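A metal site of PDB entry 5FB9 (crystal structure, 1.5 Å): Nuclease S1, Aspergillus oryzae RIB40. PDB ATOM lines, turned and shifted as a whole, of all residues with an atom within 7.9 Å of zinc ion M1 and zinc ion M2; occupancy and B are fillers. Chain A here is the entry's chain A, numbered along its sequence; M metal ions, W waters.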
ATOM      1  N   TRP A   1     -20.132   5.898   2.259  1.00  0.00           N
ATOM      2  CA  TRP A   1     -20.887   4.633   2.635  1.00  0.00           C
ATOM      3  C   TRP A   1     -19.917   3.694   3.286  1.00  0.00           C
ATOM      4  O   TRP A   1     -18.719   3.763   3.091  1.00  0.00           O
ATOM      5  CB  TRP A   1     -21.491   3.904   1.405  1.00  0.00           C
ATOM      6  CG  TRP A   1     -22.272   4.779   0.475  1.00  0.00           C
ATOM      7  CD1 TRP A   1     -21.811   5.333  -0.672  1.00  0.00           C
ATOM      8  CD2 TRP A   1     -23.603   5.231   0.613  1.00  0.00           C
ATOM      9  NE1 TRP A   1     -22.763   6.057  -1.276  1.00  0.00           N
ATOM     10  CE2 TRP A   1     -23.906   6.024  -0.517  1.00  0.00           C
ATOM     11  CE3 TRP A   1     -24.592   5.052   1.575  1.00  0.00           C
ATOM     12  CZ2 TRP A   1     -25.133   6.646  -0.687  1.00  0.00           C
ATOM     13  CZ3 TRP A   1     -25.802   5.629   1.391  1.00  0.00           C
ATOM     14  CH2 TRP A   1     -26.074   6.442   0.280  1.00  0.00           C
ATOM     15  N   GLY A   2     -20.495   2.729   3.979  1.00  0.00           N
ATOM     16  CA  GLY A   2     -19.754   1.547   4.437  1.00  0.00           C
ATOM     17  C   GLY A   2     -19.546   0.550   3.299  1.00  0.00           C
ATOM     18  O   GLY A   2     -19.908   0.820   2.128  1.00  0.00           O
ATOM     19  N   ASN A   3     -19.012  -0.622   3.631  1.00  0.00           N
ATOM     20  CA  ASN A   3     -18.629  -1.571   2.607  1.00  0.00           C
ATOM     21  C   ASN A   3     -19.795  -2.038   1.720  1.00  0.00           C
ATOM     22  O   ASN A   3     -19.658  -2.106   0.496  1.00  0.00           O
ATOM     23  CB  ASN A   3     -17.974  -2.794   3.192  1.00  0.00           C
ATOM     24  CG  ASN A   3     -16.615  -2.519   3.774  1.00  0.00           C
ATOM     25  OD1 ASN A   3     -16.069  -1.433   3.728  1.00  0.00           O
ATOM     26  ND2 ASN A   3     -16.038  -3.589   4.311  1.00  0.00           N
ATOM     27  N   GLY A   5     -22.573  -0.450   0.908  1.00  0.00           N
ATOM     28  CA  GLY A   5     -22.921   0.629  -0.034  1.00  0.00           C
ATOM     29  C   GLY A   5     -21.942   0.657  -1.200  1.00  0.00           C
ATOM     30  O   GLY A   5     -22.378   0.684  -2.369  1.00  0.00           O
ATOM     31  N   HIS A   6     -20.652   0.652  -0.926  1.00  0.00           N
ATOM     32  CA  HIS A   6     -19.646   0.668  -1.996  1.00  0.00           C
ATOM     33  C   HIS A   6     -19.694  -0.527  -2.950  1.00  0.00           C
ATOM     34  O   HIS A   6     -19.549  -0.386  -4.160  1.00  0.00           O
ATOM     35  CB  HIS A   6     -18.244   0.855  -1.431  1.00  0.00           C
ATOM     36  CG  HIS A   6     -18.038   2.225  -0.927  1.00  0.00           C
ATOM     37  ND1 HIS A   6     -17.927   3.289  -1.787  1.00  0.00           N
ATOM     38  CD2 HIS A   6     -18.092   2.768   0.313  1.00  0.00           C
ATOM     39  CE1 HIS A   6     -17.861   4.417  -1.114  1.00  0.00           C
ATOM     40  NE2 HIS A   6     -17.995   4.138   0.180  1.00  0.00           N
ATOM     41  N   ALA A  41     -14.004  -2.138  -4.247  1.00  0.00           N
ATOM     42  CA  ALA A  41     -14.783  -0.918  -3.971  1.00  0.00           C
ATOM     43  C   ALA A  41     -14.596  -0.373  -2.534  1.00  0.00           C
ATOM     44  O   ALA A  41     -14.898   0.798  -2.289  1.00  0.00           O
ATOM     45  CB  ALA A  41     -16.244  -1.198  -4.272  1.00  0.00           C
ATOM     46  N   THR A  42     -14.070  -1.219  -1.614  1.00  0.00           N
ATOM     47  CA  THR A  42     -13.818  -0.827  -0.216  1.00  0.00           C
ATOM     48  C   THR A  42     -12.362  -0.498   0.064  1.00  0.00           C
ATOM     49  O   THR A  42     -12.064  -0.050   1.151  1.00  0.00           O
ATOM     50  CB  THR A  42     -14.261  -1.911   0.784  1.00  0.00           C
ATOM     51  OG1 THR A  42     -13.291  -2.981   0.759  1.00  0.00           O
ATOM     52  CG2 THR A  42     -15.632  -2.423   0.465  1.00  0.00           C
ATOM     53  N   ALA A  44     -10.316   1.904  -0.618  1.00  0.00           N
ATOM     54  CA  ALA A  44      -9.938   3.258  -0.179  1.00  0.00           C
ATOM     55  C   ALA A  44     -10.220   3.421   1.314  1.00  0.00           C
ATOM     56  O   ALA A  44      -9.547   4.174   1.987  1.00  0.00           O
ATOM     57  CB  ALA A  44     -10.654   4.325  -0.984  1.00  0.00           C
ATOM     58  N   ASP A  45     -11.234   2.718   1.810  1.00  0.00           N
ATOM     59  CA  ASP A  45     -11.598   2.826   3.212  1.00  0.00           C
ATOM     60  C   ASP A  45     -10.654   2.063   4.132  1.00  0.00           C
ATOM     61  O   ASP A  45     -10.717   2.296   5.348  1.00  0.00           O
ATOM     62  CB  ASP A  45     -13.079   2.401   3.469  1.00  0.00           C
ATOM     63  CG  ASP A  45     -14.083   3.548   3.244  1.00  0.00           C
ATOM     64  OD1 ASP A  45     -13.641   4.714   3.058  1.00  0.00           O
ATOM     65  OD2 ASP A  45     -15.294   3.285   3.252  1.00  0.00           O
ATOM     66  N   THR A  46      -9.931   1.100   3.612  1.00  0.00           N
ATOM     67  CA  THR A  46      -8.852   0.466   4.410  1.00  0.00           C
ATOM     68  C   THR A  46      -7.560   1.239   4.265  1.00  0.00           C
ATOM     69  O   THR A  46      -6.884   1.489   5.258  1.00  0.00           O
ATOM     70  CB  THR A  46      -8.664  -0.983   4.034  1.00  0.00           C
ATOM     71  OG1 THR A  46      -9.930  -1.626   4.227  1.00  0.00           O
ATOM     72  CG2 THR A  46      -7.663  -1.637   4.950  1.00  0.00           C
ATOM     73  N   LYS A  48      -6.956   4.364   3.904  1.00  0.00           N
ATOM     74  CA  LYS A  48      -6.912   5.632   4.624  1.00  0.00           C
ATOM     75  C   LYS A  48      -6.441   5.522   6.077  1.00  0.00           C
ATOM     76  O   LYS A  48      -6.140   6.522   6.676  1.00  0.00           O
ATOM     77  CB  LYS A  48      -8.255   6.348   4.546  1.00  0.00           C
ATOM     78  CG  LYS A  48      -9.347   5.720   5.380  1.00  0.00           C
ATOM     79  CD  LYS A  48     -10.711   6.348   5.078  1.00  0.00           C
ATOM     80  CE  LYS A  48     -11.839   5.740   5.883  1.00  0.00           C
ATOM     81  NZ  LYS A  48     -13.175   6.274   5.472  1.00  0.00           N
ATOM     82  N   SER A  56      -5.119  10.479   1.930  1.00  0.00           N
ATOM     83  CA  SER A  56      -6.306  10.287   1.094  1.00  0.00           C
ATOM     84  C   SER A  56      -7.591  10.314   1.883  1.00  0.00           C
ATOM     85  O   SER A  56      -8.675  10.257   1.283  1.00  0.00           O
ATOM     86  CB  SER A  56      -6.198   9.000   0.315  1.00  0.00           C
ATOM     87  OG  SER A  56      -6.372   7.814   1.108  1.00  0.00           O
ATOM     88  N   LYS A  57      -7.527  10.421   3.212  1.00  0.00           N
ATOM     89  CA  LYS A  57      -8.744  10.616   4.005  1.00  0.00           C
ATOM     90  C   LYS A  57      -9.730  11.706   3.489  1.00  0.00           C
ATOM     91  O   LYS A  57     -10.937  11.494   3.400  1.00  0.00           O
ATOM     92  CB  LYS A  57      -8.401  10.921   5.466  1.00  0.00           C
ATOM     93  CG  LYS A  57      -7.845   9.737   6.227  1.00  0.00           C
ATOM     94  CD  LYS A  57      -7.212  10.150   7.564  1.00  0.00           C
ATOM     95  CE  LYS A  57      -8.146  11.006   8.413  1.00  0.00           C
ATOM     96  NZ  LYS A  57      -7.597  11.434   9.746  1.00  0.00           N
ATOM     97  N   TYR A  59     -10.262  12.764   0.653  1.00  0.00           N
ATOM     98  CA  TYR A  59     -10.774  12.448  -0.670  1.00  0.00           C
ATOM     99  C   TYR A  59     -12.148  11.753  -0.654  1.00  0.00           C
ATOM    100  O   TYR A  59     -12.717  11.575  -1.707  1.00  0.00           O
ATOM    101  CB  TYR A  59      -9.786  11.602  -1.480  1.00  0.00           C
ATOM    102  CG  TYR A  59      -8.389  12.189  -1.677  1.00  0.00           C
ATOM    103  CD1 TYR A  59      -8.087  13.535  -1.394  1.00  0.00           C
ATOM    104  CD2 TYR A  59      -7.416  11.430  -2.257  1.00  0.00           C
ATOM    105  CE1 TYR A  59      -6.823  14.059  -1.593  1.00  0.00           C
ATOM    106  CE2 TYR A  59      -6.137  11.943  -2.447  1.00  0.00           C
ATOM    107  CZ  TYR A  59      -5.871  13.233  -2.129  1.00  0.00           C
ATOM    108  OH  TYR A  59      -4.571  13.713  -2.390  1.00  0.00           O
ATOM    109  N   HIS A  60     -12.696  11.462   0.521  1.00  0.00           N
ATOM    110  CA  HIS A  60     -14.005  10.846   0.592  1.00  0.00           C
ATOM    111  C   HIS A  60     -15.137  11.873   0.683  1.00  0.00           C
ATOM    112  O   HIS A  60     -16.325  11.489   0.625  1.00  0.00           O
ATOM    113  CB  HIS A  60     -13.996   9.909   1.810  1.00  0.00           C
ATOM    114  CG  HIS A  60     -13.006   8.809   1.698  1.00  0.00           C
ATOM    115  ND1 HIS A  60     -13.360   7.490   1.656  1.00  0.00           N
ATOM    116  CD2 HIS A  60     -11.672   8.851   1.526  1.00  0.00           C
ATOM    117  CE1 HIS A  60     -12.272   6.753   1.471  1.00  0.00           C
ATOM    118  NE2 HIS A  60     -11.236   7.559   1.388  1.00  0.00           N
ATOM    119  N   PHE A  61     -14.780  13.138   0.811  1.00  0.00           N
ATOM    120  CA  PHE A  61     -15.711  14.200   1.200  1.00  0.00           C
ATOM    121  C   PHE A  61     -15.565  15.444   0.365  1.00  0.00           C
ATOM    122  O   PHE A  61     -14.453  15.746  -0.076  1.00  0.00           O
ATOM    123  CB  PHE A  61     -15.448  14.671   2.673  1.00  0.00           C
ATOM    124  CG  PHE A  61     -15.324  13.555   3.699  1.00  0.00           C
ATOM    125  CD1 PHE A  61     -16.467  12.842   4.079  1.00  0.00           C
ATOM    126  CD2 PHE A  61     -14.128  13.221   4.255  1.00  0.00           C
ATOM    127  CE1 PHE A  61     -16.385  11.825   5.022  1.00  0.00           C
ATOM    128  CE2 PHE A  61     -14.011  12.199   5.185  1.00  0.00           C
ATOM    129  CZ  PHE A  61     -15.153  11.500   5.578  1.00  0.00           C
ATOM    130  N   HIS A 115     -14.567   3.871  -5.702  1.00  0.00           N
ATOM    131  CA  HIS A 115     -15.017   4.223  -4.339  1.00  0.00           C
ATOM    132  C   HIS A 115     -15.628   5.589  -4.238  1.00  0.00           C
ATOM    133  O   HIS A 115     -16.696   5.783  -3.652  1.00  0.00           O
ATOM    134  CB  HIS A 115     -13.813   4.105  -3.370  1.00  0.00           C
ATOM    135  CG  HIS A 115     -14.167   4.314  -1.929  1.00  0.00           C
ATOM    136  ND1 HIS A 115     -14.611   3.294  -1.112  1.00  0.00           N
ATOM    137  CD2 HIS A 115     -14.181   5.437  -1.182  1.00  0.00           C
ATOM    138  CE1 HIS A 115     -14.855   3.799   0.092  1.00  0.00           C
ATOM    139  NE2 HIS A 115     -14.670   5.097   0.065  1.00  0.00           N
ATOM    140  N   ILE A 116     -14.917   6.566  -4.773  1.00  0.00           N
ATOM    141  CA  ILE A 116     -15.231   7.976  -4.513  1.00  0.00           C
ATOM    142  C   ILE A 116     -16.487   8.357  -5.269  1.00  0.00           C
ATOM    143  O   ILE A 116     -17.284   9.155  -4.741  1.00  0.00           O
ATOM    144  CB  ILE A 116     -14.023   8.893  -4.794  1.00  0.00           C
ATOM    145  CG1 ILE A 116     -12.885   8.543  -3.822  1.00  0.00           C
ATOM    146  CG2 ILE A 116     -14.460  10.339  -4.715  1.00  0.00           C
ATOM    147  CD1 ILE A 116     -11.592   9.303  -4.156  1.00  0.00           C
ATOM    148  N   GLY A 118     -18.961   6.475  -5.517  1.00  0.00           N
ATOM    149  CA  GLY A 118     -19.909   6.086  -4.473  1.00  0.00           C
ATOM    150  C   GLY A 118     -20.071   7.158  -3.362  1.00  0.00           C
ATOM    151  O   GLY A 118     -21.199   7.577  -3.031  1.00  0.00           O
ATOM    152  N   ASP A 119     -18.947   7.589  -2.736  1.00  0.00           N
ATOM    153  CA  ASP A 119     -19.033   8.568  -1.655  1.00  0.00           C
ATOM    154  C   ASP A 119     -19.679   9.899  -2.019  1.00  0.00           C
ATOM    155  O   ASP A 119     -20.411  10.460  -1.239  1.00  0.00           O
ATOM    156  CB  ASP A 119     -17.666   8.818  -1.048  1.00  0.00           C
ATOM    157  CG  ASP A 119     -17.306   7.815  -0.013  1.00  0.00           C
ATOM    158  OD1 ASP A 119     -18.157   7.084   0.504  1.00  0.00           O
ATOM    159  OD2 ASP A 119     -16.101   7.760   0.310  1.00  0.00           O
ATOM    160  N   ILE A 120     -19.470  10.376  -3.240  1.00  0.00           N
ATOM    161  CA  ILE A 120     -20.099  11.628  -3.699  1.00  0.00           C
ATOM    162  C   ILE A 120     -21.612  11.555  -3.614  1.00  0.00           C
ATOM    163  O   ILE A 120     -22.302  12.569  -3.498  1.00  0.00           O
ATOM    164  CB  ILE A 120     -19.586  11.970  -5.111  1.00  0.00           C
ATOM    165  CG1 ILE A 120     -18.121  12.436  -5.032  1.00  0.00           C
ATOM    166  CG2 ILE A 120     -20.440  13.017  -5.746  1.00  0.00           C
ATOM    167  CD1 ILE A 120     -17.420  12.446  -6.401  1.00  0.00           C
ATOM    168  N   GLN A 122     -23.322   9.916  -1.208  1.00  0.00           N
ATOM    169  CA  GLN A 122     -23.790   9.846   0.190  1.00  0.00           C
ATOM    170  C   GLN A 122     -23.956  11.284   0.604  1.00  0.00           C
ATOM    171  O   GLN A 122     -22.922  11.976   0.696  1.00  0.00           O
ATOM    172  CB  GLN A 122     -22.777   9.037   1.035  1.00  0.00           C
ATOM    173  CG  GLN A 122     -23.313   8.333   2.275  1.00  0.00           C
ATOM    174  CD  GLN A 122     -23.727   9.240   3.405  1.00  0.00           C
ATOM    175  OE1 GLN A 122     -24.532  10.152   3.208  1.00  0.00           O
ATOM    176  NE2 GLN A 122     -23.210   9.005   4.619  1.00  0.00           N
ATOM    177  N   HIS A 125     -21.552  12.832   3.005  1.00  0.00           N
ATOM    178  CA  HIS A 125     -20.205  13.017   2.479  1.00  0.00           C
ATOM    179  C   HIS A 125     -20.026  14.340   1.731  1.00  0.00           C
ATOM    180  O   HIS A 125     -18.903  14.666   1.322  1.00  0.00           O
ATOM    181  CB  HIS A 125     -19.784  11.843   1.611  1.00  0.00           C
ATOM    182  CG  HIS A 125     -19.282  10.677   2.390  1.00  0.00           C
ATOM    183  ND1 HIS A 125     -18.009  10.195   2.263  1.00  0.00           N
ATOM    184  CD2 HIS A 125     -19.877   9.927   3.340  1.00  0.00           C
ATOM    185  CE1 HIS A 125     -17.813   9.226   3.155  1.00  0.00           C
ATOM    186  NE2 HIS A 125     -18.941   9.026   3.783  1.00  0.00           N
ATOM    187  N   HIS A 148     -24.239  10.509  10.590  1.00  0.00           N
ATOM    188  CA  HIS A 148     -23.430  10.069   9.485  1.00  0.00           C
ATOM    189  C   HIS A 148     -23.421   8.553   9.349  1.00  0.00           C
ATOM    190  O   HIS A 148     -23.620   8.014   8.242  1.00  0.00           O
ATOM    191  CB  HIS A 148     -21.976  10.604   9.638  1.00  0.00           C
ATOM    192  CG  HIS A 148     -21.138  10.379   8.436  1.00  0.00           C
ATOM    193  ND1 HIS A 148     -20.883  11.354   7.489  1.00  0.00           N
ATOM    194  CD2 HIS A 148     -20.555   9.261   7.994  1.00  0.00           C
ATOM    195  CE1 HIS A 148     -20.163  10.815   6.514  1.00  0.00           C
ATOM    196  NE2 HIS A 148     -19.959   9.556   6.793  1.00  0.00           N
ATOM    197  N   ASP A 152     -24.309   5.905   6.313  1.00  0.00           N
ATOM    198  CA  ASP A 152     -23.268   5.110   5.718  1.00  0.00           C
ATOM    199  C   ASP A 152     -23.627   3.620   5.767  1.00  0.00           C
ATOM    200  O   ASP A 152     -23.302   2.871   4.848  1.00  0.00           O
ATOM    201  CB  ASP A 152     -21.899   5.266   6.451  1.00  0.00           C
ATOM    202  CG  ASP A 152     -21.024   6.374   5.902  1.00  0.00           C
ATOM    203  OD1 ASP A 152     -21.265   6.953   4.842  1.00  0.00           O
ATOM    204  OD2 ASP A 152     -20.062   6.630   6.616  1.00  0.00           O
ATOM    205  N   THR A 153     -24.224   3.206   6.874  1.00  0.00           N
ATOM    206  CA  THR A 153     -24.201   1.840   7.305  1.00  0.00           C
ATOM    207  C   THR A 153     -25.545   1.292   7.816  1.00  0.00           C
ATOM    208  O   THR A 153     -26.067   0.355   7.240  1.00  0.00           O
ATOM    209  CB  THR A 153     -23.094   1.666   8.359  1.00  0.00           C
ATOM    210  OG1 THR A 153     -21.809   1.888   7.732  1.00  0.00           O
ATOM    211  CG2 THR A 153     -23.056   0.299   9.006  1.00  0.00           C
HETATM  212 ZN    ZN M   1     -15.079   6.440   1.567  1.00  0.00          ZN
HETATM  213 ZN    ZN M   2     -18.169   5.397   1.766  1.00  0.00          ZN
HETATM  214 ZN    ZN M   3     -18.995   8.046   5.677  1.00  0.00          ZN
HETATM  215  O   HOH W   1     -16.465   5.665   2.595  1.00  0.00           O
HETATM  216  O   HOH W   2     -14.864   8.163   4.600  1.00  0.00           O
HETATM  217  O   HOH W   3     -18.041   6.454   4.894  1.00  0.00           O
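ND1 of His 60 lies close to OD1 of Asp 45 (3.1 Å).
A ring nitrogen (ND1) of His 125 lies within hydrogen-bond range of the backbone carbonyl oxygen (O) of His 60, 2.7 Å away.
ND1 of His 6 lies close to O of His 115 (3.3 Å).
A ring nitrogen (NE2) of His 115 lies close to the side-chain carboxylate of Asp 45, at 3.2 Å.
A ring nitrogen (ND1) of His 115 sits at hydrogen-bond distance from the backbone carbonyl oxygen of Ala 41, 2.8 Å away.
OD1 of Asp 152 sits close to N of Trp 1 (3.0 Å).
NE1 of Trp 1 sits at hydrogen-bond distance from O of Gly 118, 2.8 Å away.
The side-chain amino group of Lys 48 lies within salt-bridge range of the side-chain carboxylate of Asp 45 (2.9 Å).
Within 4 Å of zinc ion M1: His 6, Asp 45, His 60, His 115 and Asp 119.
The nearest printed residue that does not touch zinc ion M1 is His 125 (4.2 Å).
Of the 26 residues printed, 5 come within 4 Å of zinc ion M2.
Zinc ion M1 is bound by water W1 (1.9 Å), a ring nitrogen (ND1) of His 60 (2.0 Å), a ring nitrogen (NE2) of His 115 (2.1 Å) and the side-chain carboxylate of Asp 119 (2.1 Å).
Zinc ion M1 has four donor atoms within binding distance.
Slightly farther from zinc ion M1 lies OD1 of Asp 45 (2.7 Å).
Zinc ion M2 is bound by water W1.
NE2 of His 6 binds zinc ion M2 (2.0 Å).
N of Trp 1 is bound to zinc ion M2 (2.1 Å).
OD1 of Asp 119 is bound to zinc ion M2, 2.1 Å away.
O of Trp 1 is bound to zinc ion M2, at 2.2 Å.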
